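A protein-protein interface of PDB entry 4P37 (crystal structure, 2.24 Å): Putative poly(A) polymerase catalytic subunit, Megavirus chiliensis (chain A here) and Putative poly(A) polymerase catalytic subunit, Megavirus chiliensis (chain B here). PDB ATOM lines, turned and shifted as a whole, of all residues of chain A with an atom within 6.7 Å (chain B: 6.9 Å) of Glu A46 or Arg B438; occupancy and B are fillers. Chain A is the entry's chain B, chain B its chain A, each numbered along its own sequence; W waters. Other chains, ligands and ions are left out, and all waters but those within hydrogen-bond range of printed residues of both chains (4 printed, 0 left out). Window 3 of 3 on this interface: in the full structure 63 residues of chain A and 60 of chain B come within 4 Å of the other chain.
Of the 13 printed residues of chain B, 5 touch a printed residue of chain A.
Hydrophobic or aromatic side chains of chain B within 4 Å of the printed part of chain A: Val B434 and Leu B442.
Along chain B the printed residues that touch a printed residue of chain A span positions 433 to 442.
Hydrophobic or aromatic side chains of chain A within 4 Å of the printed part of chain B: Met A45 and Leu A141.
Among the printed residues, 7 pairs touch across the chains.
The side-chain carboxylate (OE2) of Glu A46 is in salt-bridge range of the guanidinium group (NH2) of Arg B438 (3.2 Å).
The backbone carbonyl oxygen of Asn A140 sits at hydrogen-bond distance from the guanidinium group of Arg B438.
The backbone carbonyl oxygen of Leu A141 is in hydrogen-bond range of the guanidinium group of Arg B441.
Among the printed residues, pairs that only touch across the chains: Met A45 with Thr B433, Glu A46 with Val B434, Leu A141 with Arg B438 and Leu A141 with Leu B442.
The side-chain hydroxyl of Ser B435 lies within hydrogen-bond range of the backbone NH of Arg B438, 3.2 Å away.
The side-chain carboxylate of Glu A46 lies within hydrogen-bond range of the side-chain amide nitrogen of Asn A140 (3.1 Å).
ND2 of Asn A140 lies within hydrogen-bond range of OE2 of Glu A51.
N of Asn A140 sits at hydrogen-bond distance from O of Pro A123, 2.9 Å away.
Water W1 bridges the backbone carbonyl oxygen (O) of Glu A46 (2.7 Å) and the backbone NH (N) of Ser B435 (3.2 Å).
Water W2 lies within hydrogen-bond range of the side-chain carboxylate of Glu A46 (2.8 Å) and the guanidinium group of Arg B438 (3.2 Å).
Water W4 lies within hydrogen-bond range of the backbone NH (N) of Thr B433 (2.9 Å) and the backbone carbonyl oxygen (O) of Val A44 (3.1 Å).
Water W3 lies within hydrogen-bond range of N of Glu A46 (3.0 Å) and O of Thr B433 (3.1 Å).
Glu A46 touches two residues of chain B.
Printed residues of chain B within 4 Å of Leu A141: Arg B438, Arg B441 and Leu B442.
Of the printed residues of chain A, Thr B433 touches Met A45.
Printed residues of chain A within 4 Å of Val B434: Glu A46.
Printed residues of chain A within 4 Å of Arg B438: Glu A46, Asn A140 and Leu A141.
Of the printed residues of chain A, Leu B442 touches Leu A141 (3.7 Å).
The nearest residue of chain B that does not touch Glu A46 is Thr B433 (4.6 Å).
The nearest residue of chain A that does not touch Arg B438 is Pro A47 (4.3 Å).
The nearest printed residue of chain A that does not touch Arg B441 is Gln A142 (4.7 Å).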
ATOM      1  N   ALA A  41      12.224  12.850  16.158  1.00  0.00           N
ATOM      2  CA  ALA A  41      11.413  13.714  17.012  1.00  0.00           C
ATOM      3  C   ALA A  41      10.317  12.914  17.717  1.00  0.00           C
ATOM      4  O   ALA A  41      10.131  13.091  18.923  1.00  0.00           O
ATOM      5  CB  ALA A  41      10.798  14.837  16.192  1.00  0.00           C
ATOM      6  N   SER A  42       9.647  11.986  16.985  1.00  0.00           N
ATOM      7  CA  SER A  42       8.578  11.124  17.529  1.00  0.00           C
ATOM      8  C   SER A  42       9.052  10.191  18.659  1.00  0.00           C
ATOM      9  O   SER A  42       8.236   9.799  19.497  1.00  0.00           O
ATOM     10  CB  SER A  42       7.892  10.320  16.421  1.00  0.00           C
ATOM     11  OG  SER A  42       8.573   9.121  16.085  1.00  0.00           O
ATOM     12  N   VAL A  44      11.829  10.984  20.847  1.00  0.00           N
ATOM     13  CA  VAL A  44      12.438  11.687  21.976  1.00  0.00           C
ATOM     14  C   VAL A  44      11.584  12.832  22.532  1.00  0.00           C
ATOM     15  O   VAL A  44      11.915  13.348  23.604  1.00  0.00           O
ATOM     16  CB  VAL A  44      13.888  12.167  21.652  1.00  0.00           C
ATOM     17  CG1 VAL A  44      14.833  10.988  21.419  1.00  0.00           C
ATOM     18  CG2 VAL A  44      13.916  13.124  20.467  1.00  0.00           C
ATOM     19  N   MET A  45      10.516  13.245  21.830  1.00  0.00           N
ATOM     20  CA  MET A  45       9.701  14.368  22.315  1.00  0.00           C
ATOM     21  C   MET A  45       8.406  13.912  22.943  1.00  0.00           C
ATOM     22  O   MET A  45       7.725  13.071  22.356  1.00  0.00           O
ATOM     23  CB  MET A  45       9.363  15.366  21.185  1.00  0.00           C
ATOM     24  CG  MET A  45      10.567  15.934  20.437  1.00  0.00           C
ATOM     25  SD  MET A  45      10.124  17.468  19.300  1.00  0.00           S
ATOM     26  CE  MET A  45       8.441  16.840  18.418  1.00  0.00           C
ATOM     27  N   GLU A  46       8.021  14.527  24.083  1.00  0.00           N
ATOM     28  CA  GLU A  46       6.755  14.261  24.773  1.00  0.00           C
ATOM     29  C   GLU A  46       5.599  14.924  23.973  1.00  0.00           C
ATOM     30  O   GLU A  46       5.715  16.110  23.653  1.00  0.00           O
ATOM     31  CB  GLU A  46       6.786  14.825  26.206  1.00  0.00           C
ATOM     32  CG  GLU A  46       5.675  14.300  27.109  1.00  0.00           C
ATOM     33  CD  GLU A  46       5.273  15.162  28.293  1.00  0.00           C
ATOM     34  OE1 GLU A  46       6.073  16.032  28.710  1.00  0.00           O
ATOM     35  OE2 GLU A  46       4.156  14.950  28.818  1.00  0.00           O
ATOM     36  N   PRO A  47       4.485  14.209  23.649  1.00  0.00           N
ATOM     37  CA  PRO A  47       4.233  12.772  23.900  1.00  0.00           C
ATOM     38  C   PRO A  47       4.973  11.905  22.878  1.00  0.00           C
ATOM     39  O   PRO A  47       4.973  12.221  21.694  1.00  0.00           O
ATOM     40  CB  PRO A  47       2.701  12.664  23.807  1.00  0.00           C
ATOM     41  CG  PRO A  47       2.277  13.781  22.870  1.00  0.00           C
ATOM     42  CD  PRO A  47       3.371  14.839  22.899  1.00  0.00           C
ATOM     43  N   THR A  48       5.647  10.850  23.328  1.00  0.00           N
ATOM     44  CA  THR A  48       6.397   9.985  22.400  1.00  0.00           C
ATOM     45  C   THR A  48       5.469   9.103  21.586  1.00  0.00           C
ATOM     46  O   THR A  48       4.305   8.941  21.954  1.00  0.00           O
ATOM     47  CB  THR A  48       7.497   9.178  23.109  1.00  0.00           C
ATOM     48  OG1 THR A  48       6.908   8.209  23.989  1.00  0.00           O
ATOM     49  CG2 THR A  48       8.504  10.065  23.834  1.00  0.00           C
ATOM     50  N   GLU A  51       3.850   6.495  23.649  1.00  0.00           N
ATOM     51  CA  GLU A  51       2.685   7.013  24.391  1.00  0.00           C
ATOM     52  C   GLU A  51       1.497   7.191  23.422  1.00  0.00           C
ATOM     53  O   GLU A  51       0.368   6.820  23.752  1.00  0.00           O
ATOM     54  CB  GLU A  51       3.006   8.362  25.090  1.00  0.00           C
ATOM     55  CG  GLU A  51       1.870   8.888  25.973  1.00  0.00           C
ATOM     56  CD  GLU A  51       1.986  10.299  26.534  1.00  0.00           C
ATOM     57  OE1 GLU A  51       3.029  10.613  27.155  1.00  0.00           O
ATOM     58  OE2 GLU A  51       0.999  11.065  26.423  1.00  0.00           O
ATOM     59  N   LYS A  52       1.774   7.744  22.227  1.00  0.00           N
ATOM     60  CA  LYS A  52       0.789   7.976  21.172  1.00  0.00           C
ATOM     61  C   LYS A  52       0.100   6.703  20.745  1.00  0.00           C
ATOM     62  O   LYS A  52      -1.124   6.670  20.701  1.00  0.00           O
ATOM     63  CB  LYS A  52       1.403   8.727  19.971  1.00  0.00           C
ATOM     64  CG  LYS A  52       1.639  10.200  20.272  1.00  0.00           C
ATOM     65  CD  LYS A  52       2.314  10.904  19.119  1.00  0.00           C
ATOM     66  CE  LYS A  52       2.502  12.377  19.378  1.00  0.00           C
ATOM     67  NZ  LYS A  52       3.390  12.996  18.362  1.00  0.00           N
ATOM     68  N   PRO A 123      -4.107  15.888  30.898  1.00  0.00           N
ATOM     69  CA  PRO A 123      -5.475  16.354  30.620  1.00  0.00           C
ATOM     70  C   PRO A 123      -6.150  15.608  29.461  1.00  0.00           C
ATOM     71  O   PRO A 123      -5.473  15.145  28.534  1.00  0.00           O
ATOM     72  CB  PRO A 123      -5.277  17.843  30.313  1.00  0.00           C
ATOM     73  CG  PRO A 123      -3.906  17.936  29.708  1.00  0.00           C
ATOM     74  CD  PRO A 123      -3.095  16.822  30.345  1.00  0.00           C
ATOM     75  N   VAL A 139      -5.592  14.491  24.172  1.00  0.00           N
ATOM     76  CA  VAL A 139      -5.047  13.770  25.324  1.00  0.00           C
ATOM     77  C   VAL A 139      -3.623  14.279  25.490  1.00  0.00           C
ATOM     78  O   VAL A 139      -2.817  14.142  24.574  1.00  0.00           O
ATOM     79  CB  VAL A 139      -5.119  12.219  25.214  1.00  0.00           C
ATOM     80  CG1 VAL A 139      -4.534  11.552  26.469  1.00  0.00           C
ATOM     81  CG2 VAL A 139      -6.561  11.745  24.978  1.00  0.00           C
ATOM     82  N   ASN A 140      -3.328  14.888  26.654  1.00  0.00           N
ATOM     83  CA  ASN A 140      -2.033  15.482  26.990  1.00  0.00           C
ATOM     84  C   ASN A 140      -1.658  16.562  25.938  1.00  0.00           C
ATOM     85  O   ASN A 140      -0.548  16.576  25.395  1.00  0.00           O
ATOM     86  CB  ASN A 140      -0.936  14.399  27.196  1.00  0.00           C
ATOM     87  CG  ASN A 140       0.344  14.895  27.822  1.00  0.00           C
ATOM     88  OD1 ASN A 140       0.387  15.947  28.450  1.00  0.00           O
ATOM     89  ND2 ASN A 140       1.423  14.145  27.662  1.00  0.00           N
ATOM     90  N   LEU A 141      -2.645  17.428  25.613  1.00  0.00           N
ATOM     91  CA  LEU A 141      -2.524  18.552  24.664  1.00  0.00           C
ATOM     92  C   LEU A 141      -2.323  18.137  23.190  1.00  0.00           C
ATOM     93  O   LEU A 141      -2.171  19.002  22.334  1.00  0.00           O
ATOM     94  CB  LEU A 141      -1.419  19.536  25.114  1.00  0.00           C
ATOM     95  CG  LEU A 141      -1.539  20.020  26.568  1.00  0.00           C
ATOM     96  CD1 LEU A 141      -0.279  20.701  27.027  1.00  0.00           C
ATOM     97  CD2 LEU A 141      -2.788  20.870  26.786  1.00  0.00           C
ATOM     98  N   GLN A 142      -2.368  16.826  22.901  1.00  0.00           N
ATOM     99  CA  GLN A 142      -2.185  16.240  21.579  1.00  0.00           C
ATOM    100  C   GLN A 142      -3.535  15.808  20.978  1.00  0.00           C
ATOM    101  O   GLN A 142      -4.313  15.142  21.658  1.00  0.00           O
ATOM    102  CB  GLN A 142      -1.220  15.035  21.695  1.00  0.00           C
ATOM    103  CG  GLN A 142      -1.090  14.142  20.448  1.00  0.00           C
ATOM    104  CD  GLN A 142      -0.390  14.788  19.280  1.00  0.00           C
ATOM    105  OE1 GLN A 142       0.677  15.402  19.401  1.00  0.00           O
ATOM    106  NE2 GLN A 142      -0.966  14.635  18.114  1.00  0.00           N
ATOM    107  N   THR B 432      16.468  17.999  25.687  1.00  0.00           N
ATOM    108  CA  THR B 432      15.023  17.767  25.657  1.00  0.00           C
ATOM    109  C   THR B 432      14.338  18.953  24.971  1.00  0.00           C
ATOM    110  O   THR B 432      14.616  20.114  25.278  1.00  0.00           O
ATOM    111  CB  THR B 432      14.489  17.569  27.103  1.00  0.00           C
ATOM    112  OG1 THR B 432      15.171  16.466  27.691  1.00  0.00           O
ATOM    113  CG2 THR B 432      12.991  17.289  27.158  1.00  0.00           C
ATOM    114  N   THR B 433      13.433  18.648  24.055  1.00  0.00           N
ATOM    115  CA  THR B 433      12.655  19.664  23.357  1.00  0.00           C
ATOM    116  C   THR B 433      11.192  19.217  23.215  1.00  0.00           C
ATOM    117  O   THR B 433      10.860  18.063  23.471  1.00  0.00           O
ATOM    118  CB  THR B 433      13.324  20.097  22.029  1.00  0.00           C
ATOM    119  OG1 THR B 433      12.769  21.352  21.633  1.00  0.00           O
ATOM    120  CG2 THR B 433      13.158  19.078  20.922  1.00  0.00           C
ATOM    121  N   VAL B 434      10.324  20.156  22.842  1.00  0.00           N
ATOM    122  CA  VAL B 434       8.911  19.908  22.581  1.00  0.00           C
ATOM    123  C   VAL B 434       8.492  20.740  21.372  1.00  0.00           C
ATOM    124  O   VAL B 434       9.081  21.804  21.120  1.00  0.00           O
ATOM    125  CB  VAL B 434       7.967  20.111  23.801  1.00  0.00           C
ATOM    126  CG1 VAL B 434       7.972  18.911  24.754  1.00  0.00           C
ATOM    127  CG2 VAL B 434       8.217  21.427  24.521  1.00  0.00           C
ATOM    128  N   SER B 435       7.487  20.245  20.627  1.00  0.00           N
ATOM    129  CA  SER B 435       6.944  20.892  19.429  1.00  0.00           C
ATOM    130  C   SER B 435       6.504  22.342  19.711  1.00  0.00           C
ATOM    131  O   SER B 435       6.208  22.687  20.862  1.00  0.00           O
ATOM    132  CB  SER B 435       5.789  20.071  18.855  1.00  0.00           C
ATOM    133  OG  SER B 435       4.650  20.072  19.704  1.00  0.00           O
ATOM    134  N   TYR B 436       6.475  23.195  18.665  1.00  0.00           N
ATOM    135  CA  TYR B 436       6.045  24.590  18.820  1.00  0.00           C
ATOM    136  C   TYR B 436       4.584  24.663  19.334  1.00  0.00           C
ATOM    137  O   TYR B 436       4.279  25.496  20.181  1.00  0.00           O
ATOM    138  CB  TYR B 436       6.214  25.355  17.484  1.00  0.00           C
ATOM    139  CG  TYR B 436       7.643  25.422  16.958  1.00  0.00           C
ATOM    140  CD1 TYR B 436       8.703  25.763  17.798  1.00  0.00           C
ATOM    141  CD2 TYR B 436       7.923  25.220  15.603  1.00  0.00           C
ATOM    142  CE1 TYR B 436      10.008  25.869  17.314  1.00  0.00           C
ATOM    143  CE2 TYR B 436       9.225  25.336  15.105  1.00  0.00           C
ATOM    144  CZ  TYR B 436      10.266  25.651  15.966  1.00  0.00           C
ATOM    145  OH  TYR B 436      11.555  25.756  15.488  1.00  0.00           O
ATOM    146  N   THR B 437       3.725  23.728  18.861  1.00  0.00           N
ATOM    147  CA  THR B 437       2.305  23.567  19.179  1.00  0.00           C
ATOM    148  C   THR B 437       2.103  23.214  20.668  1.00  0.00           C
ATOM    149  O   THR B 437       1.254  23.835  21.311  1.00  0.00           O
ATOM    150  CB  THR B 437       1.659  22.578  18.182  1.00  0.00           C
ATOM    151  OG1 THR B 437       1.680  23.163  16.874  1.00  0.00           O
ATOM    152  CG2 THR B 437       0.225  22.226  18.539  1.00  0.00           C
ATOM    153  N   ARG B 438       2.881  22.245  21.211  1.00  0.00           N
ATOM    154  CA  ARG B 438       2.819  21.843  22.624  1.00  0.00           C
ATOM    155  C   ARG B 438       3.251  22.987  23.558  1.00  0.00           C
ATOM    156  O   ARG B 438       2.558  23.277  24.540  1.00  0.00           O
ATOM    157  CB  ARG B 438       3.643  20.581  22.877  1.00  0.00           C
ATOM    158  CG  ARG B 438       3.586  20.148  24.329  1.00  0.00           C
ATOM    159  CD  ARG B 438       4.039  18.741  24.570  1.00  0.00           C
ATOM    160  NE  ARG B 438       4.051  18.483  26.011  1.00  0.00           N
ATOM    161  CZ  ARG B 438       3.001  18.073  26.720  1.00  0.00           C
ATOM    162  NH1 ARG B 438       1.841  17.828  26.121  1.00  0.00           N
ATOM    163  NH2 ARG B 438       3.111  17.876  28.026  1.00  0.00           N
ATOM    164  N   MET B 439       4.365  23.649  23.221  1.00  0.00           N
ATOM    165  CA  MET B 439       4.933  24.764  23.958  1.00  0.00           C
ATOM    166  C   MET B 439       3.945  25.926  24.026  1.00  0.00           C
ATOM    167  O   MET B 439       3.758  26.520  25.089  1.00  0.00           O
ATOM    168  CB  MET B 439       6.232  25.178  23.280  1.00  0.00           C
ATOM    169  CG  MET B 439       7.032  26.199  24.057  1.00  0.00           C
ATOM    170  SD  MET B 439       8.751  26.412  23.189  1.00  0.00           S
ATOM    171  CE  MET B 439       8.192  27.499  21.647  1.00  0.00           C
ATOM    172  N   SER B 440       3.297  26.218  22.885  1.00  0.00           N
ATOM    173  CA  SER B 440       2.286  27.261  22.718  1.00  0.00           C
ATOM    174  C   SER B 440       1.038  26.966  23.552  1.00  0.00           C
ATOM    175  O   SER B 440       0.447  27.894  24.101  1.00  0.00           O
ATOM    176  CB  SER B 440       1.904  27.384  21.245  1.00  0.00           C
ATOM    177  OG  SER B 440       0.966  28.422  21.021  1.00  0.00           O
ATOM    178  N   ARG B 441       0.630  25.688  23.642  1.00  0.00           N
ATOM    179  CA  ARG B 441      -0.548  25.280  24.421  1.00  0.00           C
ATOM    180  C   ARG B 441      -0.281  25.333  25.915  1.00  0.00           C
ATOM    181  O   ARG B 441      -1.159  25.773  26.662  1.00  0.00           O
ATOM    182  CB  ARG B 441      -1.082  23.917  23.980  1.00  0.00           C
ATOM    183  CG  ARG B 441      -1.832  24.030  22.675  1.00  0.00           C
ATOM    184  CD  ARG B 441      -2.145  22.687  22.048  1.00  0.00           C
ATOM    185  NE  ARG B 441      -2.773  22.894  20.753  1.00  0.00           N
ATOM    186  CZ  ARG B 441      -3.058  21.939  19.886  1.00  0.00           C
ATOM    187  NH1 ARG B 441      -2.781  20.671  20.169  1.00  0.00           N
ATOM    188  NH2 ARG B 441      -3.608  22.240  18.720  1.00  0.00           N
ATOM    189  N   LEU B 442       0.936  24.945  26.337  1.00  0.00           N
ATOM    190  CA  LEU B 442       1.382  25.004  27.730  1.00  0.00           C
ATOM    191  C   LEU B 442       1.465  26.450  28.196  1.00  0.00           C
ATOM    192  O   LEU B 442       1.072  26.747  29.325  1.00  0.00           O
ATOM    193  CB  LEU B 442       2.749  24.300  27.917  1.00  0.00           C
ATOM    194  CG  LEU B 442       2.732  22.772  27.927  1.00  0.00           C
ATOM    195  CD1 LEU B 442       4.083  22.220  27.562  1.00  0.00           C
ATOM    196  CD2 LEU B 442       2.280  22.229  29.282  1.00  0.00           C
ATOM    197  N   ARG B 443       1.958  27.354  27.317  1.00  0.00           N
ATOM    198  CA  ARG B 443       2.056  28.783  27.617  1.00  0.00           C
ATOM    199  C   ARG B 443       0.659  29.386  27.842  1.00  0.00           C
ATOM    200  O   ARG B 443       0.504  30.184  28.769  1.00  0.00           O
ATOM    201  CB  ARG B 443       2.818  29.523  26.497  1.00  0.00           C
ATOM    202  CG  ARG B 443       3.058  30.999  26.755  1.00  0.00           C
ATOM    203  CD  ARG B 443       4.268  31.285  27.640  1.00  0.00           C
ATOM    204  NE  ARG B 443       4.226  32.655  28.155  1.00  0.00           N
ATOM    205  CZ  ARG B 443       5.264  33.294  28.684  1.00  0.00           C
ATOM    206  NH1 ARG B 443       6.443  32.693  28.779  1.00  0.00           N
ATOM    207  NH2 ARG B 443       5.133  34.543  29.112  1.00  0.00           N
ATOM    208  N   MET B 444      -0.349  28.985  27.018  1.00  0.00           N
ATOM    209  CA  MET B 444      -1.748  29.425  27.114  1.00  0.00           C
ATOM    210  C   MET B 444      -2.337  29.028  28.458  1.00  0.00           C
ATOM    211  O   MET B 444      -3.043  29.827  29.068  1.00  0.00           O
ATOM    212  CB  MET B 444      -2.614  28.804  26.005  1.00  0.00           C
ATOM    213  CG  MET B 444      -2.353  29.365  24.632  1.00  0.00           C
ATOM    214  SD  MET B 444      -3.628  28.719  23.313  1.00  0.00           S
ATOM    215  CE  MET B 444      -2.886  29.583  21.714  1.00  0.00           C
HETATM  216  O   HOH W   1       6.123  17.452  21.312  1.00  0.00           O
HETATM  217  O   HOH W   2       6.272  18.828  28.320  1.00  0.00           O
HETATM  218  O   HOH W   3      10.142  15.929  25.651  1.00  0.00           O
HETATM  219  O   HOH W   4      13.426  15.981  22.964  1.00  0.00           O
